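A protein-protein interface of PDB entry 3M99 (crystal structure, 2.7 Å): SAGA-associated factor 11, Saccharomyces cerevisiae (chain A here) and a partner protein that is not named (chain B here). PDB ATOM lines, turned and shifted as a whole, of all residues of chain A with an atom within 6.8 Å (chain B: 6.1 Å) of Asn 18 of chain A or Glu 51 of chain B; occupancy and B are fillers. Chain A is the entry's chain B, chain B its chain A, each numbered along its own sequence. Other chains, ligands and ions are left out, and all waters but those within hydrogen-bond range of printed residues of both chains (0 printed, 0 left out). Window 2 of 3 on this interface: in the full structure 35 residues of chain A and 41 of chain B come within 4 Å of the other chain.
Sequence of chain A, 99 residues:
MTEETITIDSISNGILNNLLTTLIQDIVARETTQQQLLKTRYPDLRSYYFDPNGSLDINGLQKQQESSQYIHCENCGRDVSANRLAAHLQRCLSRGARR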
ATOM      1  N   SER A  12      18.635   9.641 -17.339  1.00  0.00           N
ATOM      2  CA  SER A  12      19.359  10.462 -18.299  1.00  0.00           C
ATOM      3  C   SER A  12      18.469  10.857 -19.475  1.00  0.00           C
ATOM      4  O   SER A  12      18.240  12.042 -19.714  1.00  0.00           O
ATOM      5  CB  SER A  12      20.604   9.728 -18.799  1.00  0.00           C
ATOM      6  OG  SER A  12      21.591   9.645 -17.785  1.00  0.00           O
ATOM      7  N   ASN A  13      17.961   9.871 -20.207  1.00  0.00           N
ATOM      8  CA  ASN A  13      17.106  10.161 -21.353  1.00  0.00           C
ATOM      9  C   ASN A  13      15.887  10.990 -20.967  1.00  0.00           C
ATOM     10  O   ASN A  13      15.312  11.700 -21.793  1.00  0.00           O
ATOM     11  CB  ASN A  13      16.695   8.875 -22.077  1.00  0.00           C
ATOM     12  CG  ASN A  13      17.715   8.446 -23.116  1.00  0.00           C
ATOM     13  OD1 ASN A  13      17.938   9.144 -24.109  1.00  0.00           O
ATOM     14  ND2 ASN A  13      18.340   7.294 -22.895  1.00  0.00           N
ATOM     15  N   GLY A  14      15.505  10.905 -19.700  1.00  0.00           N
ATOM     16  CA  GLY A  14      14.442  11.741 -19.183  1.00  0.00           C
ATOM     17  C   GLY A  14      14.922  13.173 -19.098  1.00  0.00           C
ATOM     18  O   GLY A  14      14.330  14.071 -19.701  1.00  0.00           O
ATOM     19  N   ILE A  15      16.009  13.373 -18.352  1.00  0.00           N
ATOM     20  CA  ILE A  15      16.631  14.686 -18.183  1.00  0.00           C
ATOM     21  C   ILE A  15      16.896  15.355 -19.524  1.00  0.00           C
ATOM     22  O   ILE A  15      16.730  16.566 -19.669  1.00  0.00           O
ATOM     23  CB  ILE A  15      17.971  14.585 -17.432  1.00  0.00           C
ATOM     24  CG1 ILE A  15      17.775  13.954 -16.051  1.00  0.00           C
ATOM     25  CG2 ILE A  15      18.604  15.957 -17.309  1.00  0.00           C
ATOM     26  CD1 ILE A  15      17.088  14.857 -15.049  1.00  0.00           C
ATOM     27  N   LEU A  16      17.313  14.558 -20.499  1.00  0.00           N
ATOM     28  CA  LEU A  16      17.573  15.074 -21.830  1.00  0.00           C
ATOM     29  C   LEU A  16      16.269  15.471 -22.512  1.00  0.00           C
ATOM     30  O   LEU A  16      16.140  16.598 -22.987  1.00  0.00           O
ATOM     31  CB  LEU A  16      18.324  14.043 -22.671  1.00  0.00           C
ATOM     32  CG  LEU A  16      19.003  14.592 -23.924  1.00  0.00           C
ATOM     33  CD1 LEU A  16      20.155  15.488 -23.521  1.00  0.00           C
ATOM     34  CD2 LEU A  16      19.484  13.468 -24.830  1.00  0.00           C
ATOM     35  N   ASN A  17      15.304  14.551 -22.551  1.00  0.00           N
ATOM     36  CA  ASN A  17      14.021  14.817 -23.203  1.00  0.00           C
ATOM     37  C   ASN A  17      13.359  16.044 -22.601  1.00  0.00           C
ATOM     38  O   ASN A  17      12.637  16.767 -23.281  1.00  0.00           O
ATOM     39  CB  ASN A  17      13.084  13.608 -23.102  1.00  0.00           C
ATOM     40  CG  ASN A  17      11.715  13.865 -23.735  1.00  0.00           C
ATOM     41  OD1 ASN A  17      11.609  14.122 -24.938  1.00  0.00           O
ATOM     42  ND2 ASN A  17      10.661  13.785 -22.925  1.00  0.00           N
ATOM     43  N   ASN A  18      13.615  16.272 -21.320  1.00  0.00           N
ATOM     44  CA  ASN A  18      13.061  17.421 -20.621  1.00  0.00           C
ATOM     45  C   ASN A  18      13.643  18.721 -21.136  1.00  0.00           C
ATOM     46  O   ASN A  18      12.908  19.650 -21.469  1.00  0.00           O
ATOM     47  CB  ASN A  18      13.331  17.309 -19.127  1.00  0.00           C
ATOM     48  CG  ASN A  18      12.307  16.469 -18.416  1.00  0.00           C
ATOM     49  OD1 ASN A  18      11.918  15.403 -18.890  1.00  0.00           O
ATOM     50  ND2 ASN A  18      11.862  16.943 -17.264  1.00  0.00           N
ATOM     51  N   LEU A  19      14.972  18.778 -21.182  1.00  0.00           N
ATOM     52  CA  LEU A  19      15.693  19.921 -21.738  1.00  0.00           C
ATOM     53  C   LEU A  19      15.318  20.138 -23.201  1.00  0.00           C
ATOM     54  O   LEU A  19      15.121  21.269 -23.637  1.00  0.00           O
ATOM     55  CB  LEU A  19      17.206  19.711 -21.611  1.00  0.00           C
ATOM     56  CG  LEU A  19      17.801  19.691 -20.201  1.00  0.00           C
ATOM     57  CD1 LEU A  19      19.181  19.050 -20.195  1.00  0.00           C
ATOM     58  CD2 LEU A  19      17.850  21.095 -19.615  1.00  0.00           C
ATOM     59  N   LEU A  20      15.213  19.044 -23.948  1.00  0.00           N
ATOM     60  CA  LEU A  20      14.888  19.110 -25.365  1.00  0.00           C
ATOM     61  C   LEU A  20      13.497  19.675 -25.601  1.00  0.00           C
ATOM     62  O   LEU A  20      13.299  20.521 -26.474  1.00  0.00           O
ATOM     63  CB  LEU A  20      15.012  17.730 -26.013  1.00  0.00           C
ATOM     64  CG  LEU A  20      16.409  17.378 -26.535  1.00  0.00           C
ATOM     65  CD1 LEU A  20      16.468  15.959 -27.088  1.00  0.00           C
ATOM     66  CD2 LEU A  20      16.836  18.382 -27.590  1.00  0.00           C
ATOM     67  N   THR A  21      12.534  19.208 -24.815  1.00  0.00           N
ATOM     68  CA  THR A  21      11.142  19.594 -25.013  1.00  0.00           C
ATOM     69  C   THR A  21      10.899  21.047 -24.623  1.00  0.00           C
ATOM     70  O   THR A  21      10.261  21.791 -25.365  1.00  0.00           O
ATOM     71  CB  THR A  21      10.169  18.655 -24.267  1.00  0.00           C
ATOM     72  OG1 THR A  21      10.664  18.388 -22.948  1.00  0.00           O
ATOM     73  CG2 THR A  21      10.021  17.337 -25.020  1.00  0.00           C
ATOM     74  N   THR A  22      11.416  21.447 -23.467  1.00  0.00           N
ATOM     75  CA  THR A  22      11.305  22.832 -23.033  1.00  0.00           C
ATOM     76  C   THR A  22      11.844  23.766 -24.110  1.00  0.00           C
ATOM     77  O   THR A  22      11.360  24.883 -24.286  1.00  0.00           O
ATOM     78  CB  THR A  22      12.121  23.088 -21.764  1.00  0.00           C
ATOM     79  OG1 THR A  22      12.001  21.974 -20.869  1.00  0.00           O
ATOM     80  CG2 THR A  22      11.647  24.358 -21.083  1.00  0.00           C
ATOM     81  N   LEU A  23      12.854  23.287 -24.827  1.00  0.00           N
ATOM     82  CA  LEU A  23      13.562  24.085 -25.812  1.00  0.00           C
ATOM     83  C   LEU A  23      12.781  24.109 -27.118  1.00  0.00           C
ATOM     84  O   LEU A  23      12.705  25.140 -27.794  1.00  0.00           O
ATOM     85  CB  LEU A  23      14.961  23.507 -26.036  1.00  0.00           C
ATOM     86  CG  LEU A  23      16.103  24.452 -26.401  1.00  0.00           C
ATOM     87  CD1 LEU A  23      17.407  23.674 -26.441  1.00  0.00           C
ATOM     88  CD2 LEU A  23      15.859  25.155 -27.730  1.00  0.00           C
ATOM     89  N   GLN A  25       9.511  23.671 -27.261  1.00  0.00           N
ATOM     90  CA  GLN A  25       8.294  24.407 -26.942  1.00  0.00           C
ATOM     91  C   GLN A  25       8.528  25.916 -26.876  1.00  0.00           C
ATOM     92  O   GLN A  25       7.652  26.699 -27.235  1.00  0.00           O
ATOM     93  CB  GLN A  25       7.694  23.907 -25.626  1.00  0.00           C
ATOM     94  CG  GLN A  25       7.303  22.434 -25.619  1.00  0.00           C
ATOM     95  CD  GLN A  25       6.649  22.024 -24.314  1.00  0.00           C
ATOM     96  OE1 GLN A  25       6.017  22.842 -23.643  1.00  0.00           O
ATOM     97  NE2 GLN A  25       6.801  20.756 -23.944  1.00  0.00           N
ATOM     98  N   MET B  44      10.541  27.008 -12.805  1.00  0.00           N
ATOM     99  CA  MET B  44      10.577  25.893 -13.742  1.00  0.00           C
ATOM    100  C   MET B  44      10.544  24.580 -12.987  1.00  0.00           C
ATOM    101  O   MET B  44      11.037  23.561 -13.466  1.00  0.00           O
ATOM    102  CB  MET B  44      11.832  25.959 -14.606  1.00  0.00           C
ATOM    103  CG  MET B  44      12.037  27.305 -15.281  1.00  0.00           C
ATOM    104  SD  MET B  44      13.335  27.291 -16.517  1.00  0.00           S
ATOM    105  CE  MET B  44      12.897  28.754 -17.453  1.00  0.00           C
ATOM    106  N   LYS B  45       9.979  24.634 -11.788  1.00  0.00           N
ATOM    107  CA  LYS B  45       9.693  23.452 -10.997  1.00  0.00           C
ATOM    108  C   LYS B  45       8.181  23.297 -10.923  1.00  0.00           C
ATOM    109  O   LYS B  45       7.491  24.174 -10.401  1.00  0.00           O
ATOM    110  CB  LYS B  45      10.253  23.633  -9.590  1.00  0.00           C
ATOM    111  CG  LYS B  45      10.028  22.461  -8.650  1.00  0.00           C
ATOM    112  CD  LYS B  45      10.781  22.689  -7.340  1.00  0.00           C
ATOM    113  CE  LYS B  45      10.895  21.415  -6.510  1.00  0.00           C
ATOM    114  NZ  LYS B  45      11.811  21.590  -5.339  1.00  0.00           N
ATOM    115  N   CYS B  46       7.661  22.193 -11.451  1.00  0.00           N
ATOM    116  CA  CYS B  46       6.229  21.917 -11.370  1.00  0.00           C
ATOM    117  C   CYS B  46       5.789  21.676  -9.925  1.00  0.00           C
ATOM    118  O   CYS B  46       6.406  20.890  -9.199  1.00  0.00           O
ATOM    119  CB  CYS B  46       5.863  20.708 -12.233  1.00  0.00           C
ATOM    120  SG  CYS B  46       4.093  20.526 -12.564  1.00  0.00           S
ATOM    121  N   THR B  48       3.180  20.136  -9.007  1.00  0.00           N
ATOM    122  CA  THR B  48       2.621  18.795  -8.931  1.00  0.00           C
ATOM    123  C   THR B  48       3.693  17.700  -9.079  1.00  0.00           C
ATOM    124  O   THR B  48       4.061  17.055  -8.096  1.00  0.00           O
ATOM    125  CB  THR B  48       1.532  18.600  -9.995  1.00  0.00           C
ATOM    126  OG1 THR B  48       0.633  19.718  -9.972  1.00  0.00           O
ATOM    127  CG2 THR B  48       0.768  17.318  -9.738  1.00  0.00           C
ATOM    128  N   CYS B  49       4.191  17.501 -10.301  1.00  0.00           N
ATOM    129  CA  CYS B  49       5.161  16.438 -10.596  1.00  0.00           C
ATOM    130  C   CYS B  49       6.523  16.673  -9.940  1.00  0.00           C
ATOM    131  O   CYS B  49       7.305  15.737  -9.757  1.00  0.00           O
ATOM    132  CB  CYS B  49       5.363  16.305 -12.106  1.00  0.00           C
ATOM    133  SG  CYS B  49       6.562  17.479 -12.759  1.00  0.00           S
ATOM    134  N   HIS B  50       6.803  17.930  -9.616  1.00  0.00           N
ATOM    135  CA  HIS B  50       8.058  18.318  -8.981  1.00  0.00           C
ATOM    136  C   HIS B  50       9.291  18.301  -9.902  1.00  0.00           C
ATOM    137  O   HIS B  50      10.394  18.641  -9.469  1.00  0.00           O
ATOM    138  CB  HIS B  50       8.310  17.478  -7.726  1.00  0.00           C
ATOM    139  CG  HIS B  50       7.447  17.862  -6.566  1.00  0.00           C
ATOM    140  ND1 HIS B  50       7.569  19.072  -5.918  1.00  0.00           N
ATOM    141  CD2 HIS B  50       6.448  17.194  -5.931  1.00  0.00           C
ATOM    142  CE1 HIS B  50       6.683  19.136  -4.937  1.00  0.00           C
ATOM    143  NE2 HIS B  50       5.993  18.010  -4.926  1.00  0.00           N
ATOM    144  N   GLU B  51       9.108  17.916 -11.162  1.00  0.00           N
ATOM    145  CA  GLU B  51      10.211  17.925 -12.120  1.00  0.00           C
ATOM    146  C   GLU B  51      10.518  19.352 -12.573  1.00  0.00           C
ATOM    147  O   GLU B  51       9.645  20.222 -12.568  1.00  0.00           O
ATOM    148  CB  GLU B  51       9.905  17.035 -13.340  1.00  0.00           C
ATOM    149  CG  GLU B  51      10.059  15.528 -13.100  1.00  0.00           C
ATOM    150  CD  GLU B  51       9.885  14.695 -14.369  1.00  0.00           C
ATOM    151  OE1 GLU B  51      10.742  14.787 -15.281  1.00  0.00           O
ATOM    152  OE2 GLU B  51       8.894  13.931 -14.443  1.00  0.00           O
ATOM    153  N   ILE B  52      11.765  19.596 -12.952  1.00  0.00           N
ATOM    154  CA  ILE B  52      12.116  20.882 -13.526  1.00  0.00           C
ATOM    155  C   ILE B  52      12.317  20.696 -15.018  1.00  0.00           C
ATOM    156  O   ILE B  52      12.770  19.641 -15.466  1.00  0.00           O
ATOM    157  CB  ILE B  52      13.383  21.458 -12.903  1.00  0.00           C
ATOM    158  CG1 ILE B  52      14.599  20.676 -13.383  1.00  0.00           C
ATOM    159  CG2 ILE B  52      13.291  21.446 -11.372  1.00  0.00           C
ATOM    160  CD1 ILE B  52      15.855  21.001 -12.614  1.00  0.00           C
ATOM    161  N   ASN B  53      11.964  21.721 -15.786  1.00  0.00           N
ATOM    162  CA  ASN B  53      11.968  21.629 -17.239  1.00  0.00           C
ATOM    163  C   ASN B  53      11.284  20.367 -17.738  1.00  0.00           C
ATOM    164  O   ASN B  53      11.802  19.704 -18.637  1.00  0.00           O
ATOM    165  CB  ASN B  53      13.393  21.675 -17.783  1.00  0.00           C
ATOM    166  CG  ASN B  53      14.057  23.012 -17.564  1.00  0.00           C
ATOM    167  OD1 ASN B  53      13.456  24.065 -17.783  1.00  0.00           O
ATOM    168  ND2 ASN B  53      15.307  22.980 -17.135  1.00  0.00           N
ATOM    169  N   SER B  54      10.144  20.022 -17.141  1.00  0.00           N
ATOM    170  CA  SER B  54       9.315  18.952 -17.683  1.00  0.00           C
ATOM    171  C   SER B  54       9.151  19.279 -19.160  1.00  0.00           C
ATOM    172  O   SER B  54       9.938  18.833 -19.998  1.00  0.00           O
ATOM    173  CB  SER B  54       7.957  18.894 -16.987  1.00  0.00           C
ATOM    174  OG  SER B  54       7.266  17.708 -17.330  1.00  0.00           O
ATOM    175  N   GLY B  55       8.141  20.076 -19.483  1.00  0.00           N
ATOM    176  CA  GLY B  55       8.140  20.770 -20.757  1.00  0.00           C
ATOM    177  C   GLY B  55       8.343  22.225 -20.402  1.00  0.00           C
ATOM    178  O   GLY B  55       9.094  22.542 -19.477  1.00  0.00           O
ATOM    179  N   THR B  57       7.215  25.334 -18.385  1.00  0.00           N
ATOM    180  CA  THR B  57       6.525  25.493 -17.118  1.00  0.00           C
ATOM    181  C   THR B  57       5.856  26.862 -17.106  1.00  0.00           C
ATOM    182  O   THR B  57       6.348  27.804 -17.723  1.00  0.00           O
ATOM    183  CB  THR B  57       7.477  25.348 -15.922  1.00  0.00           C
ATOM    184  OG1 THR B  57       8.018  24.019 -15.892  1.00  0.00           O
ATOM    185  CG2 THR B  57       6.732  25.608 -14.625  1.00  0.00           C
ATOM    186  N   CYS B  68       3.951  22.203 -15.088  1.00  0.00           N
ATOM    187  CA  CYS B  68       4.631  21.776 -16.306  1.00  0.00           C
ATOM    188  C   CYS B  68       3.657  21.624 -17.464  1.00  0.00           C
ATOM    189  O   CYS B  68       2.545  22.155 -17.430  1.00  0.00           O
ATOM    190  CB  CYS B  68       5.309  20.434 -16.079  1.00  0.00           C
ATOM    191  SG  CYS B  68       4.124  19.079 -15.958  1.00  0.00           S
ATOM    192  N   ASN B  70       4.385  18.567 -20.136  1.00  0.00           N
ATOM    193  CA  ASN B  70       4.475  17.184 -20.604  1.00  0.00           C
ATOM    194  C   ASN B  70       3.572  16.231 -19.834  1.00  0.00           C
ATOM    195  O   ASN B  70       3.170  15.189 -20.353  1.00  0.00           O
ATOM    196  CB  ASN B  70       5.914  16.679 -20.528  1.00  0.00           C
ATOM    197  CG  ASN B  70       6.846  17.443 -21.432  1.00  0.00           C
ATOM    198  OD1 ASN B  70       6.423  18.293 -22.218  1.00  0.00           O
ATOM    199  ND2 ASN B  70       8.128  17.139 -21.332  1.00  0.00           N
ATOM    200  N   HIS B  71       3.275  16.584 -18.587  1.00  0.00           N
ATOM    201  CA  HIS B  71       2.330  15.829 -17.778  1.00  0.00           C
ATOM    202  C   HIS B  71       1.070  16.667 -17.616  1.00  0.00           C
ATOM    203  O   HIS B  71       0.259  16.425 -16.723  1.00  0.00           O
ATOM    204  CB  HIS B  71       2.920  15.504 -16.405  1.00  0.00           C
ATOM    205  CG  HIS B  71       4.272  14.869 -16.457  1.00  0.00           C
ATOM    206  ND1 HIS B  71       5.430  15.552 -16.147  1.00  0.00           N
ATOM    207  CD2 HIS B  71       4.657  13.609 -16.779  1.00  0.00           C
ATOM    208  CE1 HIS B  71       6.466  14.744 -16.279  1.00  0.00           C
ATOM    209  NE2 HIS B  71       6.028  13.562 -16.661  1.00  0.00           N
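Leu 16 of chain A touches none of the printed residues of chain B. Asn 17 of chain A touches none of the printed residues of chain B. Asn 18 of chain A touches just these residues of chain B: Glu 51, Ile 52, Asn 53 and Ser 54. Printed residues of chain B within 4 Å of Gln 25 of chain A: Gly 55 (3.5 Å) and Asn 70 (3.0 Å). Glu 51 of chain B touches just one residue of chain A: Asn 18 (3.1 Å). Of the printed residues of chain A, Ile 52 of chain B touches Asn 18. Of the printed residues of chain A, Ser 54 of chain B touches Asn 18 (3.3 Å), Thr 21 (3.1 Å) and Thr 22 (3.9 Å). Printed residues of chain A within 4 Å of Gly 55 of chain B: Thr 22 and Gln 25. The nearest residue of chain B that does not touch Asn 18 of chain A is Asn 70 of chain B (4.8 Å).
N of Gly 55 of chain B sits close to ND2 of Asn 70 of chain B (3.5 Å). OG1 of Thr 21 of chain A sits at hydrogen-bond distance from O of Asn 17 of chain A, at 2.6 Å. The side-chain hydroxyl of Thr 21 of chain A sits at hydrogen-bond distance from the backbone carbonyl oxygen of Asn 18 of chain A, at 3.0 Å. OG1 of Thr 22 of chain A is in hydrogen-bond range of O of Asn 18 of chain A (2.6 Å). The backbone carbonyl oxygen (O) of Gly 14 of chain A lies close to the side-chain amide oxygen (OD1) of Asn 18 of chain A (2.9 Å). The side-chain sulfur of Cys 49 of chain B lies close to the backbone NH of Glu 51 of chain B (3.0 Å).
Among the printed residues, pairs that only touch across the chains: Thr 22 of chain A with Ser 54 of chain B (3.9 Å) and Gln 25 of chain A with Gly 55 of chain B (3.5 Å).
The side-chain amide nitrogen (ND2) of Asn 18 of chain A sits close to the backbone carbonyl oxygen (O) of Asn 53 of chain B (3.1 Å). The side-chain carboxylate of Glu 51 of chain B lies within hydrogen-bond range of the side-chain amide nitrogen of Asn 18 of chain A (3.1 Å). The backbone carbonyl oxygen of Ser 54 of chain B lies close to the backbone carbonyl oxygen of Asn 18 of chain A. NE2 of Gln 25 of chain A is in hydrogen-bond range of OD1 of Asn 70 of chain B (3.0 Å). The backbone carbonyl oxygen (O) of Gly 55 of chain B sits at hydrogen-bond distance from the side-chain hydroxyl (OG1) of Thr 22 of chain A, 3.3 Å away. The side-chain amide nitrogen (ND2) of Asn 18 of chain A is in hydrogen-bond range of the backbone carbonyl oxygen (O) of Ile 52 of chain B, at 3.4 Å. The backbone carbonyl oxygen of Ser 54 of chain B is in hydrogen-bond range of the side-chain hydroxyl of Thr 21 of chain A, at 3.1 Å. The side-chain hydroxyl of Thr 22 of chain A is in hydrogen-bond range of the backbone carbonyl oxygen of Asn 53 of chain B, 3.2 Å away. OG1 of Thr 21 of chain A lies within hydrogen-bond range of ND2 of Asn 70 of chain B (3.3 Å).
Printed residues of chain B that touch a printed residue of chain A: Glu 51, Ile 52, Asn 53, Ser 54, Gly 55 and Asn 70. Among the printed residues, 11 pairs touch across the chains.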
